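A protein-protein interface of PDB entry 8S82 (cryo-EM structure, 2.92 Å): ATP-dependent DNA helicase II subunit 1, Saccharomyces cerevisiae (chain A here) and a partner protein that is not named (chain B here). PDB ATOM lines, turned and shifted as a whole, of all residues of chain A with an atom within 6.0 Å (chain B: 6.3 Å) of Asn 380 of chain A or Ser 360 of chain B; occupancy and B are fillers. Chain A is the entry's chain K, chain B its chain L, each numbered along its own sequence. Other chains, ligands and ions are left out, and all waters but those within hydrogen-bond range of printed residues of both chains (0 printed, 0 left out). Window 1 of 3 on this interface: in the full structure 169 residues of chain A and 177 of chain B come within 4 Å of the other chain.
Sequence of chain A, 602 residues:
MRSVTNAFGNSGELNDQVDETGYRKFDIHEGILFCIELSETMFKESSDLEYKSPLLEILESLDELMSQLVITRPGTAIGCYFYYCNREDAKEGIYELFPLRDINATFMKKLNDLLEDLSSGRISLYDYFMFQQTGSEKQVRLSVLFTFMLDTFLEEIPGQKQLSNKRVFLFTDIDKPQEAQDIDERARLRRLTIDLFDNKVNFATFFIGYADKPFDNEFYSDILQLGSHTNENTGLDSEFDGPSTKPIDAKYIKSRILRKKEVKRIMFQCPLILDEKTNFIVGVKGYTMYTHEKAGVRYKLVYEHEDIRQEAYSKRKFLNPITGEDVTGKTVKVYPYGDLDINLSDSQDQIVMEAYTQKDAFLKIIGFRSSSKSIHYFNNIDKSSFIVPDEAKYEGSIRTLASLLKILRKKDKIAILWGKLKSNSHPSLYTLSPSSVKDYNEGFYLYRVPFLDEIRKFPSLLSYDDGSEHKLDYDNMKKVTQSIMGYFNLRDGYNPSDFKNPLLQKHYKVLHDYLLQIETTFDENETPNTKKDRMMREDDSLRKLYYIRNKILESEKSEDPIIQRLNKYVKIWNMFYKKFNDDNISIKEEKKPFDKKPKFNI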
ATOM      1  N   HIS A 376      -2.170  17.046 -20.309  1.00  0.00           N
ATOM      2  CA  HIS A 376      -1.360  15.979 -20.874  1.00  0.00           C
ATOM      3  C   HIS A 376       0.103  16.361 -20.734  1.00  0.00           C
ATOM      4  O   HIS A 376       0.445  17.538 -20.595  1.00  0.00           O
ATOM      5  CB  HIS A 376      -1.683  15.724 -22.351  1.00  0.00           C
ATOM      6  CG  HIS A 376      -3.140  15.560 -22.642  1.00  0.00           C
ATOM      7  ND1 HIS A 376      -3.763  16.204 -23.687  1.00  0.00           N
ATOM      8  CD2 HIS A 376      -4.091  14.809 -22.041  1.00  0.00           C
ATOM      9  CE1 HIS A 376      -5.038  15.866 -23.712  1.00  0.00           C
ATOM     10  NE2 HIS A 376      -5.265  15.021 -22.723  1.00  0.00           N
ATOM     11  N   TYR A 377       0.971  15.351 -20.782  1.00  0.00           N
ATOM     12  CA  TYR A 377       2.399  15.611 -20.662  1.00  0.00           C
ATOM     13  C   TYR A 377       3.096  15.647 -22.016  1.00  0.00           C
ATOM     14  O   TYR A 377       4.228  16.133 -22.111  1.00  0.00           O
ATOM     15  CB  TYR A 377       3.039  14.569 -19.748  1.00  0.00           C
ATOM     16  CG  TYR A 377       2.574  14.694 -18.320  1.00  0.00           C
ATOM     17  CD1 TYR A 377       3.183  15.586 -17.449  1.00  0.00           C
ATOM     18  CD2 TYR A 377       1.513  13.941 -17.847  1.00  0.00           C
ATOM     19  CE1 TYR A 377       2.757  15.714 -16.147  1.00  0.00           C
ATOM     20  CE2 TYR A 377       1.077  14.064 -16.545  1.00  0.00           C
ATOM     21  CZ  TYR A 377       1.704  14.952 -15.700  1.00  0.00           C
ATOM     22  OH  TYR A 377       1.276  15.077 -14.401  1.00  0.00           O
ATOM     23  N   PHE A 378       2.442  15.163 -23.067  1.00  0.00           N
ATOM     24  CA  PHE A 378       3.019  15.148 -24.403  1.00  0.00           C
ATOM     25  C   PHE A 378       2.691  16.394 -25.211  1.00  0.00           C
ATOM     26  O   PHE A 378       3.203  16.543 -26.323  1.00  0.00           O
ATOM     27  CB  PHE A 378       2.548  13.909 -25.163  1.00  0.00           C
ATOM     28  CG  PHE A 378       1.056  13.719 -25.162  1.00  0.00           C
ATOM     29  CD1 PHE A 378       0.471  12.761 -24.357  1.00  0.00           C
ATOM     30  CD2 PHE A 378       0.241  14.487 -25.974  1.00  0.00           C
ATOM     31  CE1 PHE A 378      -0.893  12.578 -24.358  1.00  0.00           C
ATOM     32  CE2 PHE A 378      -1.122  14.307 -25.975  1.00  0.00           C
ATOM     33  CZ  PHE A 378      -1.688  13.351 -25.166  1.00  0.00           C
ATOM     34  N   ASN A 379       1.853  17.288 -24.687  1.00  0.00           N
ATOM     35  CA  ASN A 379       1.419  18.455 -25.444  1.00  0.00           C
ATOM     36  C   ASN A 379       1.847  19.752 -24.772  1.00  0.00           C
ATOM     37  O   ASN A 379       1.100  20.733 -24.782  1.00  0.00           O
ATOM     38  CB  ASN A 379      -0.099  18.436 -25.623  1.00  0.00           C
ATOM     39  CG  ASN A 379      -0.840  18.459 -24.310  1.00  0.00           C
ATOM     40  OD1 ASN A 379      -0.241  18.329 -23.246  1.00  0.00           O
ATOM     41  ND2 ASN A 379      -2.152  18.620 -24.375  1.00  0.00           N
ATOM     42  N   ASN A 380       3.041  19.770 -24.192  1.00  0.00           N
ATOM     43  CA  ASN A 380       3.606  20.977 -23.611  1.00  0.00           C
ATOM     44  C   ASN A 380       4.387  21.720 -24.682  1.00  0.00           C
ATOM     45  O   ASN A 380       5.073  21.108 -25.503  1.00  0.00           O
ATOM     46  CB  ASN A 380       4.510  20.664 -22.419  1.00  0.00           C
ATOM     47  CG  ASN A 380       5.053  21.916 -21.763  1.00  0.00           C
ATOM     48  OD1 ASN A 380       4.346  22.602 -21.032  1.00  0.00           O
ATOM     49  ND2 ASN A 380       6.323  22.210 -22.007  1.00  0.00           N
ATOM     50  N   ILE A 381       4.255  23.041 -24.683  1.00  0.00           N
ATOM     51  CA  ILE A 381       4.861  23.869 -25.715  1.00  0.00           C
ATOM     52  C   ILE A 381       5.549  25.066 -25.074  1.00  0.00           C
ATOM     53  O   ILE A 381       6.353  25.753 -25.715  1.00  0.00           O
ATOM     54  CB  ILE A 381       3.796  24.309 -26.734  1.00  0.00           C
ATOM     55  CG1 ILE A 381       4.442  24.952 -27.955  1.00  0.00           C
ATOM     56  CG2 ILE A 381       2.798  25.257 -26.091  1.00  0.00           C
ATOM     57  CD1 ILE A 381       3.459  25.346 -28.987  1.00  0.00           C
ATOM     58  N   ASP A 382       5.259  25.315 -23.800  1.00  0.00           N
ATOM     59  CA  ASP A 382       5.703  26.545 -23.162  1.00  0.00           C
ATOM     60  C   ASP A 382       5.971  26.282 -21.687  1.00  0.00           C
ATOM     61  O   ASP A 382       5.895  25.149 -21.209  1.00  0.00           O
ATOM     62  CB  ASP A 382       4.668  27.658 -23.341  1.00  0.00           C
ATOM     63  CG  ASP A 382       5.269  29.039 -23.212  1.00  0.00           C
ATOM     64  OD1 ASP A 382       6.503  29.136 -23.042  1.00  0.00           O
ATOM     65  OD2 ASP A 382       4.509  30.025 -23.278  1.00  0.00           O
ATOM     66  N   LYS A 383       6.290  27.359 -20.976  1.00  0.00           N
ATOM     67  CA  LYS A 383       6.607  27.336 -19.555  1.00  0.00           C
ATOM     68  C   LYS A 383       5.352  27.645 -18.754  1.00  0.00           C
ATOM     69  O   LYS A 383       4.650  28.617 -19.045  1.00  0.00           O
ATOM     70  CB  LYS A 383       7.692  28.364 -19.236  1.00  0.00           C
ATOM     71  CG  LYS A 383       8.922  27.803 -18.572  1.00  0.00           C
ATOM     72  CD  LYS A 383      10.154  28.566 -19.011  1.00  0.00           C
ATOM     73  CE  LYS A 383       9.945  30.061 -18.893  1.00  0.00           C
ATOM     74  NZ  LYS A 383      11.138  30.817 -19.363  1.00  0.00           N
ATOM     75  N   SER A 384       5.081  26.829 -17.742  1.00  0.00           N
ATOM     76  CA  SER A 384       3.917  27.047 -16.902  1.00  0.00           C
ATOM     77  C   SER A 384       4.101  28.306 -16.062  1.00  0.00           C
ATOM     78  O   SER A 384       5.215  28.792 -15.855  1.00  0.00           O
ATOM     79  CB  SER A 384       3.676  25.838 -16.005  1.00  0.00           C
ATOM     80  OG  SER A 384       2.588  26.059 -15.135  1.00  0.00           O
ATOM     81  N   TYR A 447      -1.043  26.674 -17.828  1.00  0.00           N
ATOM     82  CA  TYR A 447      -0.297  26.091 -18.931  1.00  0.00           C
ATOM     83  C   TYR A 447      -0.873  26.615 -20.238  1.00  0.00           C
ATOM     84  O   TYR A 447      -2.024  27.043 -20.290  1.00  0.00           O
ATOM     85  CB  TYR A 447      -0.365  24.564 -18.921  1.00  0.00           C
ATOM     86  CG  TYR A 447      -0.301  23.949 -17.549  1.00  0.00           C
ATOM     87  CD1 TYR A 447       0.848  24.034 -16.783  1.00  0.00           C
ATOM     88  CD2 TYR A 447      -1.386  23.269 -17.027  1.00  0.00           C
ATOM     89  CE1 TYR A 447       0.911  23.469 -15.530  1.00  0.00           C
ATOM     90  CE2 TYR A 447      -1.332  22.700 -15.776  1.00  0.00           C
ATOM     91  CZ  TYR A 447      -0.180  22.801 -15.033  1.00  0.00           C
ATOM     92  OH  TYR A 447      -0.128  22.232 -13.785  1.00  0.00           O
ATOM     93  N   ARG A 448      -0.072  26.579 -21.294  1.00  0.00           N
ATOM     94  CA  ARG A 448      -0.510  27.006 -22.614  1.00  0.00           C
ATOM     95  C   ARG A 448      -0.934  25.789 -23.425  1.00  0.00           C
ATOM     96  O   ARG A 448      -0.274  24.747 -23.385  1.00  0.00           O
ATOM     97  CB  ARG A 448       0.600  27.767 -23.341  1.00  0.00           C
ATOM     98  CG  ARG A 448       0.355  27.954 -24.818  1.00  0.00           C
ATOM     99  CD  ARG A 448       0.138  29.404 -25.161  1.00  0.00           C
ATOM    100  NE  ARG A 448       1.356  30.188 -25.012  1.00  0.00           N
ATOM    101  CZ  ARG A 448       2.278  30.316 -25.954  1.00  0.00           C
ATOM    102  NH1 ARG A 448       2.164  29.701 -27.120  1.00  0.00           N
ATOM    103  NH2 ARG A 448       3.342  31.078 -25.722  1.00  0.00           N
ATOM    104  N   PRO A 450      -1.358  24.017 -26.970  1.00  0.00           N
ATOM    105  CA  PRO A 450      -0.785  24.168 -28.314  1.00  0.00           C
ATOM    106  C   PRO A 450      -1.869  24.256 -29.379  1.00  0.00           C
ATOM    107  O   PRO A 450      -2.833  23.487 -29.374  1.00  0.00           O
ATOM    108  CB  PRO A 450       0.064  22.902 -28.482  1.00  0.00           C
ATOM    109  CG  PRO A 450      -0.531  21.930 -27.546  1.00  0.00           C
ATOM    110  CD  PRO A 450      -1.018  22.717 -26.373  1.00  0.00           C
ATOM    111  N   THR B 250       5.801  19.537 -30.708  1.00  0.00           N
ATOM    112  CA  THR B 250       5.079  20.799 -30.662  1.00  0.00           C
ATOM    113  C   THR B 250       6.110  21.909 -30.754  1.00  0.00           C
ATOM    114  O   THR B 250       7.138  21.852 -30.080  1.00  0.00           O
ATOM    115  CB  THR B 250       4.254  20.955 -29.377  1.00  0.00           C
ATOM    116  OG1 THR B 250       5.128  20.999 -28.246  1.00  0.00           O
ATOM    117  CG2 THR B 250       3.277  19.807 -29.210  1.00  0.00           C
ATOM    118  N   ARG B 355       3.065  18.732 -13.160  1.00  0.00           N
ATOM    119  CA  ARG B 355       2.857  19.203 -14.520  1.00  0.00           C
ATOM    120  C   ARG B 355       3.639  20.463 -14.852  1.00  0.00           C
ATOM    121  O   ARG B 355       4.045  20.631 -16.006  1.00  0.00           O
ATOM    122  CB  ARG B 355       1.366  19.464 -14.767  1.00  0.00           C
ATOM    123  CG  ARG B 355       0.729  18.543 -15.794  1.00  0.00           C
ATOM    124  CD  ARG B 355       0.699  19.168 -17.182  1.00  0.00           C
ATOM    125  NE  ARG B 355       1.890  19.960 -17.446  1.00  0.00           N
ATOM    126  CZ  ARG B 355       2.187  20.506 -18.614  1.00  0.00           C
ATOM    127  NH1 ARG B 355       1.423  20.326 -19.676  1.00  0.00           N
ATOM    128  NH2 ARG B 355       3.277  21.258 -18.716  1.00  0.00           N
ATOM    129  N   PHE B 357       6.563  21.201 -14.043  1.00  0.00           N
ATOM    130  CA  PHE B 357       7.986  20.940 -14.230  1.00  0.00           C
ATOM    131  C   PHE B 357       8.386  21.050 -15.695  1.00  0.00           C
ATOM    132  O   PHE B 357       9.422  21.641 -16.016  1.00  0.00           O
ATOM    133  CB  PHE B 357       8.346  19.561 -13.684  1.00  0.00           C
ATOM    134  CG  PHE B 357       8.725  19.562 -12.234  1.00  0.00           C
ATOM    135  CD1 PHE B 357       8.798  20.743 -11.526  1.00  0.00           C
ATOM    136  CD2 PHE B 357       9.024  18.381 -11.585  1.00  0.00           C
ATOM    137  CE1 PHE B 357       9.148  20.743 -10.196  1.00  0.00           C
ATOM    138  CE2 PHE B 357       9.376  18.378 -10.257  1.00  0.00           C
ATOM    139  CZ  PHE B 357       9.437  19.561  -9.562  1.00  0.00           C
ATOM    140  N   LEU B 358       7.580  20.491 -16.598  1.00  0.00           N
ATOM    141  CA  LEU B 358       7.890  20.503 -18.023  1.00  0.00           C
ATOM    142  C   LEU B 358       7.975  21.936 -18.531  1.00  0.00           C
ATOM    143  O   LEU B 358       6.995  22.682 -18.455  1.00  0.00           O
ATOM    144  CB  LEU B 358       6.839  19.717 -18.805  1.00  0.00           C
ATOM    145  CG  LEU B 358       6.383  18.387 -18.201  1.00  0.00           C
ATOM    146  CD1 LEU B 358       5.388  17.711 -19.115  1.00  0.00           C
ATOM    147  CD2 LEU B 358       7.558  17.467 -17.925  1.00  0.00           C
ATOM    148  N   THR B 359       9.138  22.333 -19.044  1.00  0.00           N
ATOM    149  CA  THR B 359       9.396  23.725 -19.384  1.00  0.00           C
ATOM    150  C   THR B 359       9.916  23.917 -20.802  1.00  0.00           C
ATOM    151  O   THR B 359      10.595  24.910 -21.068  1.00  0.00           O
ATOM    152  CB  THR B 359      10.385  24.335 -18.387  1.00  0.00           C
ATOM    153  OG1 THR B 359      11.099  25.405 -19.014  1.00  0.00           O
ATOM    154  CG2 THR B 359      11.369  23.297 -17.908  1.00  0.00           C
ATOM    155  N   SER B 360       9.612  23.003 -21.720  1.00  0.00           N
ATOM    156  CA  SER B 360      10.065  23.165 -23.096  1.00  0.00           C
ATOM    157  C   SER B 360       9.156  22.451 -24.082  1.00  0.00           C
ATOM    158  O   SER B 360       8.275  21.683 -23.688  1.00  0.00           O
ATOM    159  CB  SER B 360      11.491  22.648 -23.265  1.00  0.00           C
ATOM    160  OG  SER B 360      11.491  21.254 -23.513  1.00  0.00           O
ATOM    161  N   GLU B 361       9.386  22.696 -25.369  1.00  0.00           N
ATOM    162  CA  GLU B 361       8.639  22.072 -26.450  1.00  0.00           C
ATOM    163  C   GLU B 361       8.926  20.578 -26.524  1.00  0.00           C
ATOM    164  O   GLU B 361      10.063  20.148 -26.312  1.00  0.00           O
ATOM    165  CB  GLU B 361       8.990  22.762 -27.764  1.00  0.00           C
ATOM    166  CG  GLU B 361       9.000  24.271 -27.641  1.00  0.00           C
ATOM    167  CD  GLU B 361       9.645  24.961 -28.819  1.00  0.00           C
ATOM    168  OE1 GLU B 361       8.909  25.512 -29.662  1.00  0.00           O
ATOM    169  OE2 GLU B 361      10.889  24.956 -28.902  1.00  0.00           O
ATOM    170  N   SER B 362       7.909  19.782 -26.829  1.00  0.00           N
ATOM    171  CA  SER B 362       8.020  18.331 -26.845  1.00  0.00           C
ATOM    172  C   SER B 362       8.742  17.862 -28.102  1.00  0.00           C
ATOM    173  O   SER B 362       8.824  18.596 -29.090  1.00  0.00           O
ATOM    174  CB  SER B 362       6.635  17.695 -26.766  1.00  0.00           C
ATOM    175  OG  SER B 362       5.923  18.175 -25.644  1.00  0.00           O
ATOM    176  N   LEU B 433       9.551  13.715 -25.418  1.00  0.00           N
ATOM    177  CA  LEU B 433      10.599  14.258 -24.576  1.00  0.00           C
ATOM    178  C   LEU B 433      10.364  15.741 -24.328  1.00  0.00           C
ATOM    179  O   LEU B 433      10.216  16.533 -25.263  1.00  0.00           O
ATOM    180  CB  LEU B 433      11.956  14.033 -25.243  1.00  0.00           C
ATOM    181  CG  LEU B 433      13.274  14.481 -24.622  1.00  0.00           C
ATOM    182  CD1 LEU B 433      14.359  13.528 -25.052  1.00  0.00           C
ATOM    183  CD2 LEU B 433      13.628  15.891 -25.054  1.00  0.00           C
ATOM    184  N   CYS B 434      10.329  16.106 -23.050  1.00  0.00           N
ATOM    185  CA  CYS B 434      10.105  17.489 -22.652  1.00  0.00           C
ATOM    186  C   CYS B 434      11.036  17.839 -21.501  1.00  0.00           C
ATOM    187  O   CYS B 434      11.147  17.095 -20.529  1.00  0.00           O
ATOM    188  CB  CYS B 434       8.647  17.722 -22.257  1.00  0.00           C
ATOM    189  SG  CYS B 434       7.877  16.287 -21.480  1.00  0.00           S
ATOM    190  N   ARG B 435      11.696  18.987 -21.615  1.00  0.00           N
ATOM    191  CA  ARG B 435      12.759  19.351 -20.690  1.00  0.00           C
ATOM    192  C   ARG B 435      12.225  19.612 -19.284  1.00  0.00           C
ATOM    193  O   ARG B 435      11.105  20.092 -19.096  1.00  0.00           O
ATOM    194  CB  ARG B 435      13.513  20.573 -21.213  1.00  0.00           C
ATOM    195  CG  ARG B 435      13.843  21.619 -20.179  1.00  0.00           C
ATOM    196  CD  ARG B 435      14.911  22.559 -20.683  1.00  0.00           C
ATOM    197  NE  ARG B 435      15.257  23.563 -19.685  1.00  0.00           N
ATOM    198  CZ  ARG B 435      16.024  23.336 -18.628  1.00  0.00           C
ATOM    199  NH1 ARG B 435      16.528  22.138 -18.383  1.00  0.00           N
ATOM    200  NH2 ARG B 435      16.292  24.335 -17.795  1.00  0.00           N
ATOM    201  N   LEU B 436      13.044  19.271 -18.297  1.00  0.00           N
ATOM    202  CA  LEU B 436      12.804  19.454 -16.877  1.00  0.00           C
ATOM    203  C   LEU B 436      13.773  20.490 -16.329  1.00  0.00           C
ATOM    204  O   LEU B 436      14.877  20.660 -16.859  1.00  0.00           O
ATOM    205  CB  LEU B 436      12.980  18.132 -16.117  1.00  0.00           C
ATOM    206  CG  LEU B 436      11.918  17.050 -16.294  1.00  0.00           C
ATOM    207  CD1 LEU B 436      12.386  15.744 -15.684  1.00  0.00           C
ATOM    208  CD2 LEU B 436      10.605  17.482 -15.679  1.00  0.00           C
ATOM    209  N   TYR B 495      -1.403  13.244 -32.347  1.00  0.00           N
ATOM    210  CA  TYR B 495      -0.310  13.464 -33.280  1.00  0.00           C
ATOM    211  C   TYR B 495      -0.629  12.708 -34.560  1.00  0.00           C
ATOM    212  O   TYR B 495      -0.914  11.508 -34.521  1.00  0.00           O
ATOM    213  CB  TYR B 495       1.022  13.008 -32.691  1.00  0.00           C
ATOM    214  CG  TYR B 495       1.539  13.905 -31.598  1.00  0.00           C
ATOM    215  CD1 TYR B 495       2.006  15.176 -31.885  1.00  0.00           C
ATOM    216  CD2 TYR B 495       1.563  13.482 -30.282  1.00  0.00           C
ATOM    217  CE1 TYR B 495       2.482  15.996 -30.895  1.00  0.00           C
ATOM    218  CE2 TYR B 495       2.036  14.297 -29.284  1.00  0.00           C
ATOM    219  CZ  TYR B 495       2.494  15.551 -29.597  1.00  0.00           C
ATOM    220  OH  TYR B 495       2.968  16.370 -28.603  1.00  0.00           O
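The side-chain amide nitrogen of Asn 380 of chain A is in hydrogen-bond range of the backbone carbonyl oxygen of Ser 360 of chain B (2.6 Å).
The guanidinium group (NH2) of Arg 355 of chain B is in hydrogen-bond range of the side-chain amide oxygen (OD1) of Asn 380 of chain A (2.9 Å).
The backbone carbonyl oxygen (O) of Asn 380 of chain A lies within hydrogen-bond range of the side-chain hydroxyl (OG) of Ser 362 of chain B (3.1 Å).
O of Tyr 377 of chain A is in hydrogen-bond range of SG of Cys 434 of chain B, 3.7 Å away.
The guanidinium group (NH1) of Arg 355 of chain B lies within hydrogen-bond range of the backbone carbonyl oxygen (O) of His 376 of chain A (3.1 Å).
The side-chain hydroxyl of Ser 362 of chain B lies within hydrogen-bond range of the backbone carbonyl oxygen of Phe 378 of chain A, at 3.2 Å.
The backbone carbonyl oxygen of Asn 380 of chain A sits at hydrogen-bond distance from the side-chain hydroxyl of Thr 250 of chain B, 2.7 Å away.
OH of Tyr 495 of chain B sits close to O of Phe 378 of chain A (2.3 Å).
The side-chain amide oxygen (OD1) of Asn 380 of chain A lies close to the backbone carbonyl oxygen (O) of Asp 382 of chain A.
N of Thr 359 of chain B is in hydrogen-bond range of O of Arg 435 of chain B, at 3.0 Å.
OD2 of Asp 382 of chain A is in salt-bridge range of NH2 of Arg 448 of chain A (2.9 Å).
The backbone NH (N) of Arg 435 of chain B lies within hydrogen-bond range of the side-chain hydroxyl (OG) of Ser 360 of chain B.
OD1 of Asn 379 of chain A lies close to O of His 376 of chain A.
OG1 of Thr 250 of chain B lies within hydrogen-bond range of N of Ser 362 of chain B (3.4 Å).
CE1 of Tyr 377 of chain A touches CG of Arg 355 of chain B, at 3.5 Å.
Tyr 377 of chain A touches Leu 358 of chain B (CD1 to CD1, 3.5 Å).
Leu 358 of chain B touches Asn 380 of chain A (O to ND2, 3.6 Å).
CA of Glu 361 of chain B touches O of Asn 380 of chain A, at 3.8 Å.
Ile 381 of chain A touches Thr 250 of chain B.
O of Ile 381 of chain A touches CG of Glu 361 of chain B (3.6 Å).
Leu 358 of chain B touches Asp 382 of chain A.
Thr 359 of chain B touches Lys 383 of chain A (OG1 to CG, 3.3 Å).
OH of Tyr 447 of chain A touches CB of Arg 355 of chain B (3.3 Å).
Of chain B, only Thr 250 (2.7 Å), Arg 355 (2.9 Å), Leu 358 (3.6 Å), Ser 360 (2.6 Å), Glu 361 (3.8 Å) and Ser 362 (3.1 Å) come within 4 Å of Asn 380 of chain A.
Ser 360 of chain B touches one residue of chain A.
Printed residues of chain B within 4 Å of Phe 378 of chain A: Ser 362 (3.2 Å) and Tyr 495 (2.3 Å).
Of the printed residues of chain B, Asp 382 of chain A touches Leu 358 (3.9 Å).
Of the printed residues of chain A, Thr 250 of chain B touches Asn 380 and Ile 381.
Printed residues of chain A within 4 Å of Thr 359 of chain B: Lys 383.
Of the printed residues of chain B, Lys 383 of chain A touches Thr 359.
The nearest residue of chain B that does not touch Asn 380 of chain A is Thr 359 of chain B (4.1 Å).
Of the 12 printed residues of chain A, 8 touch a printed residue of chain B.
Of the 13 printed residues of chain B, 9 touch a printed residue of chain A.
Hydrophobic or aromatic side chains of chain B within 4 Å of the printed part of chain A: Leu 358 and Tyr 495.
Among the printed residues, no Asp or Glu carboxylate lies within 4 Å of a Lys or Arg side-chain nitrogen of the other chain.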
